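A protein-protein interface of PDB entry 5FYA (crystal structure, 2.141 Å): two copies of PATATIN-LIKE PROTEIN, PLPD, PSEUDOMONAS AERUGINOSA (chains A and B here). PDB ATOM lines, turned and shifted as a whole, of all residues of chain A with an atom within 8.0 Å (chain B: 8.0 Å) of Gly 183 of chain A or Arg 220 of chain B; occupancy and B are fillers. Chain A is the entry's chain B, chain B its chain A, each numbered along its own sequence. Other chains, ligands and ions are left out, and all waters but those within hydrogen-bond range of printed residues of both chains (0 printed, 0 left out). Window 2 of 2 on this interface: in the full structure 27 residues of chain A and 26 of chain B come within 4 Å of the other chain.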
ATOM      1  N   ASP A 148      26.259 -20.978 -18.192  1.00  0.00           N
ATOM      2  CA  ASP A 148      25.992 -19.660 -18.743  1.00  0.00           C
ATOM      3  C   ASP A 148      26.102 -19.810 -20.251  1.00  0.00           C
ATOM      4  O   ASP A 148      27.200 -19.964 -20.784  1.00  0.00           O
ATOM      5  CB  ASP A 148      27.010 -18.637 -18.228  1.00  0.00           C
ATOM      6  CG  ASP A 148      26.709 -17.212 -18.690  1.00  0.00           C
ATOM      7  OD1 ASP A 148      26.345 -17.010 -19.869  1.00  0.00           O
ATOM      8  OD2 ASP A 148      26.843 -16.283 -17.868  1.00  0.00           O
ATOM      9  N   ILE A 149      24.966 -19.768 -20.937  1.00  0.00           N
ATOM     10  CA  ILE A 149      24.940 -20.024 -22.374  1.00  0.00           C
ATOM     11  C   ILE A 149      25.606 -18.906 -23.186  1.00  0.00           C
ATOM     12  O   ILE A 149      25.994 -19.110 -24.333  1.00  0.00           O
ATOM     13  CB  ILE A 149      23.498 -20.287 -22.880  1.00  0.00           C
ATOM     14  CG1 ILE A 149      23.510 -20.890 -24.288  1.00  0.00           C
ATOM     15  CG2 ILE A 149      22.671 -19.013 -22.831  1.00  0.00           C
ATOM     16  CD1 ILE A 149      24.283 -22.191 -24.398  1.00  0.00           C
ATOM     17  N   ALA A 150      25.758 -17.730 -22.587  1.00  0.00           N
ATOM     18  CA  ALA A 150      26.404 -16.619 -23.283  1.00  0.00           C
ATOM     19  C   ALA A 150      27.927 -16.747 -23.298  1.00  0.00           C
ATOM     20  O   ALA A 150      28.580 -16.382 -24.274  1.00  0.00           O
ATOM     21  CB  ALA A 150      25.986 -15.291 -22.674  1.00  0.00           C
ATOM     22  N   THR A 151      28.488 -17.272 -22.213  1.00  0.00           N
ATOM     23  CA  THR A 151      29.938 -17.346 -22.060  1.00  0.00           C
ATOM     24  C   THR A 151      30.452 -18.776 -22.127  1.00  0.00           C
ATOM     25  O   THR A 151      31.604 -19.012 -22.488  1.00  0.00           O
ATOM     26  CB  THR A 151      30.388 -16.740 -20.721  1.00  0.00           C
ATOM     27  OG1 THR A 151      29.850 -17.513 -19.641  1.00  0.00           O
ATOM     28  CG2 THR A 151      29.909 -15.304 -20.600  1.00  0.00           C
ATOM     29  N   VAL A 179      16.685 -19.998 -18.325  1.00  0.00           N
ATOM     30  CA  VAL A 179      16.224 -19.108 -17.272  1.00  0.00           C
ATOM     31  C   VAL A 179      17.259 -18.023 -16.991  1.00  0.00           C
ATOM     32  O   VAL A 179      18.448 -18.195 -17.276  1.00  0.00           O
ATOM     33  CB  VAL A 179      15.922 -19.877 -15.975  1.00  0.00           C
ATOM     34  CG1 VAL A 179      15.075 -21.104 -16.273  1.00  0.00           C
ATOM     35  CG2 VAL A 179      17.207 -20.281 -15.292  1.00  0.00           C
ATOM     36  N   GLU A 180      16.796 -16.904 -16.441  1.00  0.00           N
ATOM     37  CA  GLU A 180      17.674 -15.796 -16.092  1.00  0.00           C
ATOM     38  C   GLU A 180      17.885 -15.720 -14.587  1.00  0.00           C
ATOM     39  O   GLU A 180      16.924 -15.678 -13.822  1.00  0.00           O
ATOM     40  CB  GLU A 180      17.096 -14.470 -16.587  1.00  0.00           C
ATOM     41  CG  GLU A 180      17.016 -14.343 -18.096  1.00  0.00           C
ATOM     42  CD  GLU A 180      16.672 -12.935 -18.548  1.00  0.00           C
ATOM     43  OE1 GLU A 180      16.419 -12.070 -17.680  1.00  0.00           O
ATOM     44  OE2 GLU A 180      16.662 -12.692 -19.773  1.00  0.00           O
ATOM     45  N   ILE A 181      19.145 -15.707 -14.164  1.00  0.00           N
ATOM     46  CA  ILE A 181      19.480 -15.507 -12.756  1.00  0.00           C
ATOM     47  C   ILE A 181      20.686 -14.580 -12.636  1.00  0.00           C
ATOM     48  O   ILE A 181      21.732 -14.830 -13.241  1.00  0.00           O
ATOM     49  CB  ILE A 181      19.780 -16.839 -12.024  1.00  0.00           C
ATOM     50  CG1 ILE A 181      18.578 -17.784 -12.093  1.00  0.00           C
ATOM     51  CG2 ILE A 181      20.154 -16.576 -10.574  1.00  0.00           C
ATOM     52  CD1 ILE A 181      18.860 -19.179 -11.585  1.00  0.00           C
ATOM     53  N   ASP A 182      20.524 -13.508 -11.862  1.00  0.00           N
ATOM     54  CA  ASP A 182      21.583 -12.525 -11.631  1.00  0.00           C
ATOM     55  C   ASP A 182      22.211 -12.009 -12.924  1.00  0.00           C
ATOM     56  O   ASP A 182      23.434 -11.900 -13.029  1.00  0.00           O
ATOM     57  CB  ASP A 182      22.662 -13.089 -10.700  1.00  0.00           C
ATOM     58  CG  ASP A 182      22.203 -13.168  -9.253  1.00  0.00           C
ATOM     59  OD1 ASP A 182      21.447 -12.272  -8.813  1.00  0.00           O
ATOM     60  OD2 ASP A 182      22.601 -14.124  -8.554  1.00  0.00           O
ATOM     61  N   GLY A 183      21.370 -11.703 -13.906  1.00  0.00           N
ATOM     62  CA  GLY A 183      21.836 -11.155 -15.165  1.00  0.00           C
ATOM     63  C   GLY A 183      22.418 -12.185 -16.115  1.00  0.00           C
ATOM     64  O   GLY A 183      22.918 -11.834 -17.184  1.00  0.00           O
ATOM     65  N   ARG A 184      22.355 -13.457 -15.738  1.00  0.00           N
ATOM     66  CA  ARG A 184      22.899 -14.509 -16.590  1.00  0.00           C
ATOM     67  C   ARG A 184      21.820 -15.405 -17.188  1.00  0.00           C
ATOM     68  O   ARG A 184      20.882 -15.807 -16.502  1.00  0.00           O
ATOM     69  CB  ARG A 184      23.931 -15.345 -15.831  1.00  0.00           C
ATOM     70  CG  ARG A 184      25.152 -14.551 -15.406  1.00  0.00           C
ATOM     71  CD  ARG A 184      26.274 -15.451 -14.928  1.00  0.00           C
ATOM     72  NE  ARG A 184      26.478 -15.353 -13.488  1.00  0.00           N
ATOM     73  CZ  ARG A 184      27.614 -15.668 -12.878  1.00  0.00           C
ATOM     74  NH1 ARG A 184      28.650 -16.096 -13.585  1.00  0.00           N
ATOM     75  NH2 ARG A 184      27.715 -15.548 -11.559  1.00  0.00           N
ATOM     76  N   LEU A 185      21.968 -15.705 -18.475  1.00  0.00           N
ATOM     77  CA  LEU A 185      21.081 -16.630 -19.166  1.00  0.00           C
ATOM     78  C   LEU A 185      21.633 -18.044 -19.023  1.00  0.00           C
ATOM     79  O   LEU A 185      22.762 -18.321 -19.428  1.00  0.00           O
ATOM     80  CB  LEU A 185      20.971 -16.249 -20.640  1.00  0.00           C
ATOM     81  CG  LEU A 185      19.889 -16.962 -21.447  1.00  0.00           C
ATOM     82  CD1 LEU A 185      18.523 -16.672 -20.852  1.00  0.00           C
ATOM     83  CD2 LEU A 185      19.949 -16.530 -22.901  1.00  0.00           C
ATOM     84  N   LEU A 186      20.835 -18.942 -18.452  1.00  0.00           N
ATOM     85  CA  LEU A 186      21.347 -20.239 -18.025  1.00  0.00           C
ATOM     86  C   LEU A 186      20.623 -21.436 -18.633  1.00  0.00           C
ATOM     87  O   LEU A 186      19.395 -21.468 -18.703  1.00  0.00           O
ATOM     88  CB  LEU A 186      21.288 -20.343 -16.499  1.00  0.00           C
ATOM     89  CG  LEU A 186      21.962 -19.211 -15.724  1.00  0.00           C
ATOM     90  CD1 LEU A 186      21.432 -19.158 -14.304  1.00  0.00           C
ATOM     91  CD2 LEU A 186      23.473 -19.381 -15.729  1.00  0.00           C
ATOM     92  N   LEU B 217      31.473 -16.357 -29.968  1.00  0.00           N
ATOM     93  CA  LEU B 217      30.251 -16.684 -29.246  1.00  0.00           C
ATOM     94  C   LEU B 217      29.241 -15.563 -29.443  1.00  0.00           C
ATOM     95  O   LEU B 217      29.604 -14.453 -29.830  1.00  0.00           O
ATOM     96  CB  LEU B 217      30.550 -16.877 -27.756  1.00  0.00           C
ATOM     97  CG  LEU B 217      31.440 -18.070 -27.383  1.00  0.00           C
ATOM     98  CD1 LEU B 217      32.078 -17.877 -26.012  1.00  0.00           C
ATOM     99  CD2 LEU B 217      30.643 -19.367 -27.420  1.00  0.00           C
ATOM    100  N   ARG B 218      27.971 -15.850 -29.187  1.00  0.00           N
ATOM    101  CA  ARG B 218      26.931 -14.838 -29.310  1.00  0.00           C
ATOM    102  C   ARG B 218      26.627 -14.214 -27.950  1.00  0.00           C
ATOM    103  O   ARG B 218      26.773 -14.864 -26.916  1.00  0.00           O
ATOM    104  CB  ARG B 218      25.663 -15.448 -29.908  1.00  0.00           C
ATOM    105  CG  ARG B 218      25.891 -16.162 -31.229  1.00  0.00           C
ATOM    106  CD  ARG B 218      24.685 -17.004 -31.620  1.00  0.00           C
ATOM    107  NE  ARG B 218      23.531 -16.186 -31.984  1.00  0.00           N
ATOM    108  CZ  ARG B 218      23.253 -15.797 -33.225  1.00  0.00           C
ATOM    109  NH1 ARG B 218      24.046 -16.150 -34.227  1.00  0.00           N
ATOM    110  NH2 ARG B 218      22.180 -15.055 -33.466  1.00  0.00           N
ATOM    111  N   ASP B 219      26.216 -12.951 -27.956  1.00  0.00           N
ATOM    112  CA  ASP B 219      25.789 -12.291 -26.730  1.00  0.00           C
ATOM    113  C   ASP B 219      24.432 -12.847 -26.319  1.00  0.00           C
ATOM    114  O   ASP B 219      23.727 -13.437 -27.136  1.00  0.00           O
ATOM    115  CB  ASP B 219      25.702 -10.777 -26.925  1.00  0.00           C
ATOM    116  CG  ASP B 219      27.024 -10.164 -27.342  1.00  0.00           C
ATOM    117  OD1 ASP B 219      27.921 -10.039 -26.482  1.00  0.00           O
ATOM    118  OD2 ASP B 219      27.163  -9.799 -28.529  1.00  0.00           O
ATOM    119  N   ARG B 220      24.062 -12.649 -25.058  1.00  0.00           N
ATOM    120  CA  ARG B 220      22.813 -13.200 -24.533  1.00  0.00           C
ATOM    121  C   ARG B 220      21.570 -12.625 -25.213  1.00  0.00           C
ATOM    122  O   ARG B 220      20.461 -13.125 -25.021  1.00  0.00           O
ATOM    123  CB  ARG B 220      22.732 -12.999 -23.020  1.00  0.00           C
ATOM    124  CG  ARG B 220      23.113 -11.610 -22.559  1.00  0.00           C
ATOM    125  CD  ARG B 220      22.623 -11.376 -21.149  1.00  0.00           C
ATOM    126  NE  ARG B 220      21.195 -11.660 -21.049  1.00  0.00           N
ATOM    127  CZ  ARG B 220      20.466 -11.454 -19.960  1.00  0.00           C
ATOM    128  NH1 ARG B 220      21.026 -10.957 -18.866  1.00  0.00           N
ATOM    129  NH2 ARG B 220      19.172 -11.743 -19.966  1.00  0.00           N
ATOM    130  N   LYS B 221      21.762 -11.574 -26.002  1.00  0.00           N
ATOM    131  CA  LYS B 221      20.680 -10.988 -26.782  1.00  0.00           C
ATOM    132  C   LYS B 221      20.483 -11.749 -28.090  1.00  0.00           C
ATOM    133  O   LYS B 221      19.393 -11.743 -28.663  1.00  0.00           O
ATOM    134  CB  LYS B 221      20.963  -9.509 -27.058  1.00  0.00           C
ATOM    135  CG  LYS B 221      22.359  -9.230 -27.596  1.00  0.00           C
ATOM    136  CD  LYS B 221      22.616  -7.736 -27.726  1.00  0.00           C
ATOM    137  CE  LYS B 221      24.058  -7.453 -28.118  1.00  0.00           C
ATOM    138  NZ  LYS B 221      24.425  -8.093 -29.413  1.00  0.00           N
ATOM    139  N   ASP B 222      21.541 -12.408 -28.554  1.00  0.00           N
ATOM    140  CA  ASP B 222      21.486 -13.176 -29.795  1.00  0.00           C
ATOM    141  C   ASP B 222      21.260 -14.662 -29.535  1.00  0.00           C
ATOM    142  O   ASP B 222      21.524 -15.501 -30.398  1.00  0.00           O
ATOM    143  CB  ASP B 222      22.764 -12.976 -30.613  1.00  0.00           C
ATOM    144  CG  ASP B 222      22.899 -11.567 -31.147  1.00  0.00           C
ATOM    145  OD1 ASP B 222      21.876 -10.850 -31.198  1.00  0.00           O
ATOM    146  OD2 ASP B 222      24.024 -11.178 -31.521  1.00  0.00           O
ATOM    147  N   LEU B 223      20.778 -14.982 -28.340  1.00  0.00           N
ATOM    148  CA  LEU B 223      20.459 -16.358 -27.981  1.00  0.00           C
ATOM    149  C   LEU B 223      18.972 -16.451 -27.667  1.00  0.00           C
ATOM    150  O   LEU B 223      18.579 -16.898 -26.589  1.00  0.00           O
ATOM    151  CB  LEU B 223      21.291 -16.802 -26.778  1.00  0.00           C
ATOM    152  CG  LEU B 223      22.810 -16.735 -26.955  1.00  0.00           C
ATOM    153  CD1 LEU B 223      23.522 -16.934 -25.627  1.00  0.00           C
ATOM    154  CD2 LEU B 223      23.284 -17.761 -27.978  1.00  0.00           C
ATOM    155  N   SER B 224      18.155 -16.025 -28.624  1.00  0.00           N
ATOM    156  CA  SER B 224      16.716 -15.884 -28.419  1.00  0.00           C
ATOM    157  C   SER B 224      15.918 -17.150 -28.722  1.00  0.00           C
ATOM    158  O   SER B 224      14.815 -17.328 -28.205  1.00  0.00           O
ATOM    159  CB  SER B 224      16.184 -14.721 -29.260  1.00  0.00           C
ATOM    160  OG  SER B 224      16.588 -14.849 -30.613  1.00  0.00           O
ATOM    161  N   THR B 225      16.469 -18.028 -29.557  1.00  0.00           N
ATOM    162  CA  THR B 225      15.761 -19.248 -29.942  1.00  0.00           C
ATOM    163  C   THR B 225      16.518 -20.522 -29.566  1.00  0.00           C
ATOM    164  O   THR B 225      17.686 -20.474 -29.176  1.00  0.00           O
ATOM    165  CB  THR B 225      15.448 -19.275 -31.455  1.00  0.00           C
ATOM    166  OG1 THR B 225      16.670 -19.328 -32.201  1.00  0.00           O
ATOM    167  CG2 THR B 225      14.658 -18.039 -31.859  1.00  0.00           C
ATOM    168  N   GLN B 232      25.196 -22.332 -30.213  1.00  0.00           N
ATOM    169  CA  GLN B 232      26.136 -21.793 -29.242  1.00  0.00           C
ATOM    170  C   GLN B 232      26.903 -22.929 -28.575  1.00  0.00           C
ATOM    171  O   GLN B 232      28.121 -22.846 -28.399  1.00  0.00           O
ATOM    172  CB  GLN B 232      25.408 -20.958 -28.195  1.00  0.00           C
ATOM    173  CG  GLN B 232      26.325 -20.300 -27.180  1.00  0.00           C
ATOM    174  CD  GLN B 232      26.932 -19.006 -27.685  1.00  0.00           C
ATOM    175  OE1 GLN B 232      26.950 -18.737 -28.885  1.00  0.00           O
ATOM    176  NE2 GLN B 232      27.425 -18.188 -26.762  1.00  0.00           N
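Leu 223 of chain B touches Ile 149 of chain A. Ala 150 of chain A touches Arg 218 of chain B (O to O, 3.5 Å). CB of Arg 220 of chain B touches CB of Ala 150 of chain A (3.995 Å). Ala 150 of chain A touches Leu 223 of chain B (CA to CD1, 3.7 Å). CD1 of Leu 217 of chain B touches O of Thr 151 of chain A, 3.7 Å away. Leu 185 of chain A touches Leu 223 of chain B.
No position is printed for both chains. Of the 10 pairs that touch across the chains among the printed residues, none has its exchanged pair printed and touching as well.
Of the 12 printed residues of chain A, 6 touch a printed residue of chain B. Hydrophobic or aromatic side chains of chain A within 4 Å of the printed part of chain B: Ile 149, Ala 150 and Leu 185. Printed residues of chain B that touch a printed residue of chain A: Leu 217, Arg 218, Arg 220, Leu 223 and Gln 232. Among the printed residues, 10 pairs touch across the chains.
Of chain B, only Arg 220 (2.7 Å) comes within 4 Å of Gly 183 of chain A. Of the printed residues of chain A, Arg 220 of chain B touches Ala 150 (3.995 Å), Glu 180 (2.7 Å) and Gly 183 (2.7 Å). Printed residues of chain B within 4 Å of Ala 150 of chain A: Arg 218 (3.5 Å), Arg 220 (3.995 Å), Leu 223 (3.7 Å) and Gln 232 (3.3 Å). Printed residues of chain A within 4 Å of Gln 232 of chain B: Ile 149 (3.0 Å) and Ala 150 (3.3 Å). Printed residues of chain B within 4 Å of Leu 185 of chain A: Leu 223. Of the printed residues of chain A, Arg 218 of chain B touches Ala 150. Arg 184 of chain A touches none of the printed residues of chain B. The nearest printed residue of chain B that does not touch Thr 151 of chain A is Gln 232 of chain B (4.8 Å).
The guanidinium group of Arg 220 of chain B is in salt-bridge range of the side-chain carboxylate of Glu 180 of chain A. O of Gly 183 of chain A sits at hydrogen-bond distance from NH1 of Arg 220 of chain B, 2.7 Å away. O of Ile 149 of chain A sits at hydrogen-bond distance from NE2 of Gln 232 of chain B (3.0 Å). O of Ala 150 of chain A sits at hydrogen-bond distance from NE2 of Gln 232 of chain B (3.3 Å).
The backbone carbonyl oxygen (O) of Asp 222 of chain B is in hydrogen-bond range of the guanidinium group (NE) of Arg 218 of chain B (2.6 Å). N of Arg 218 of chain B is in hydrogen-bond range of OE1 of Gln 232 of chain B, 3.1 Å away. The backbone NH of Ala 150 of chain A is in hydrogen-bond range of the side-chain carboxylate of Asp 148 of chain A, 2.9 Å away. The side-chain carboxylate (OD1) of Asp 148 of chain A is in hydrogen-bond range of the backbone NH (N) of Thr 151 of chain A (3.2 Å). The backbone carbonyl oxygen of Leu 185 of chain A is in hydrogen-bond range of the backbone NH of Ile 149 of chain A, at 3.0 Å.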
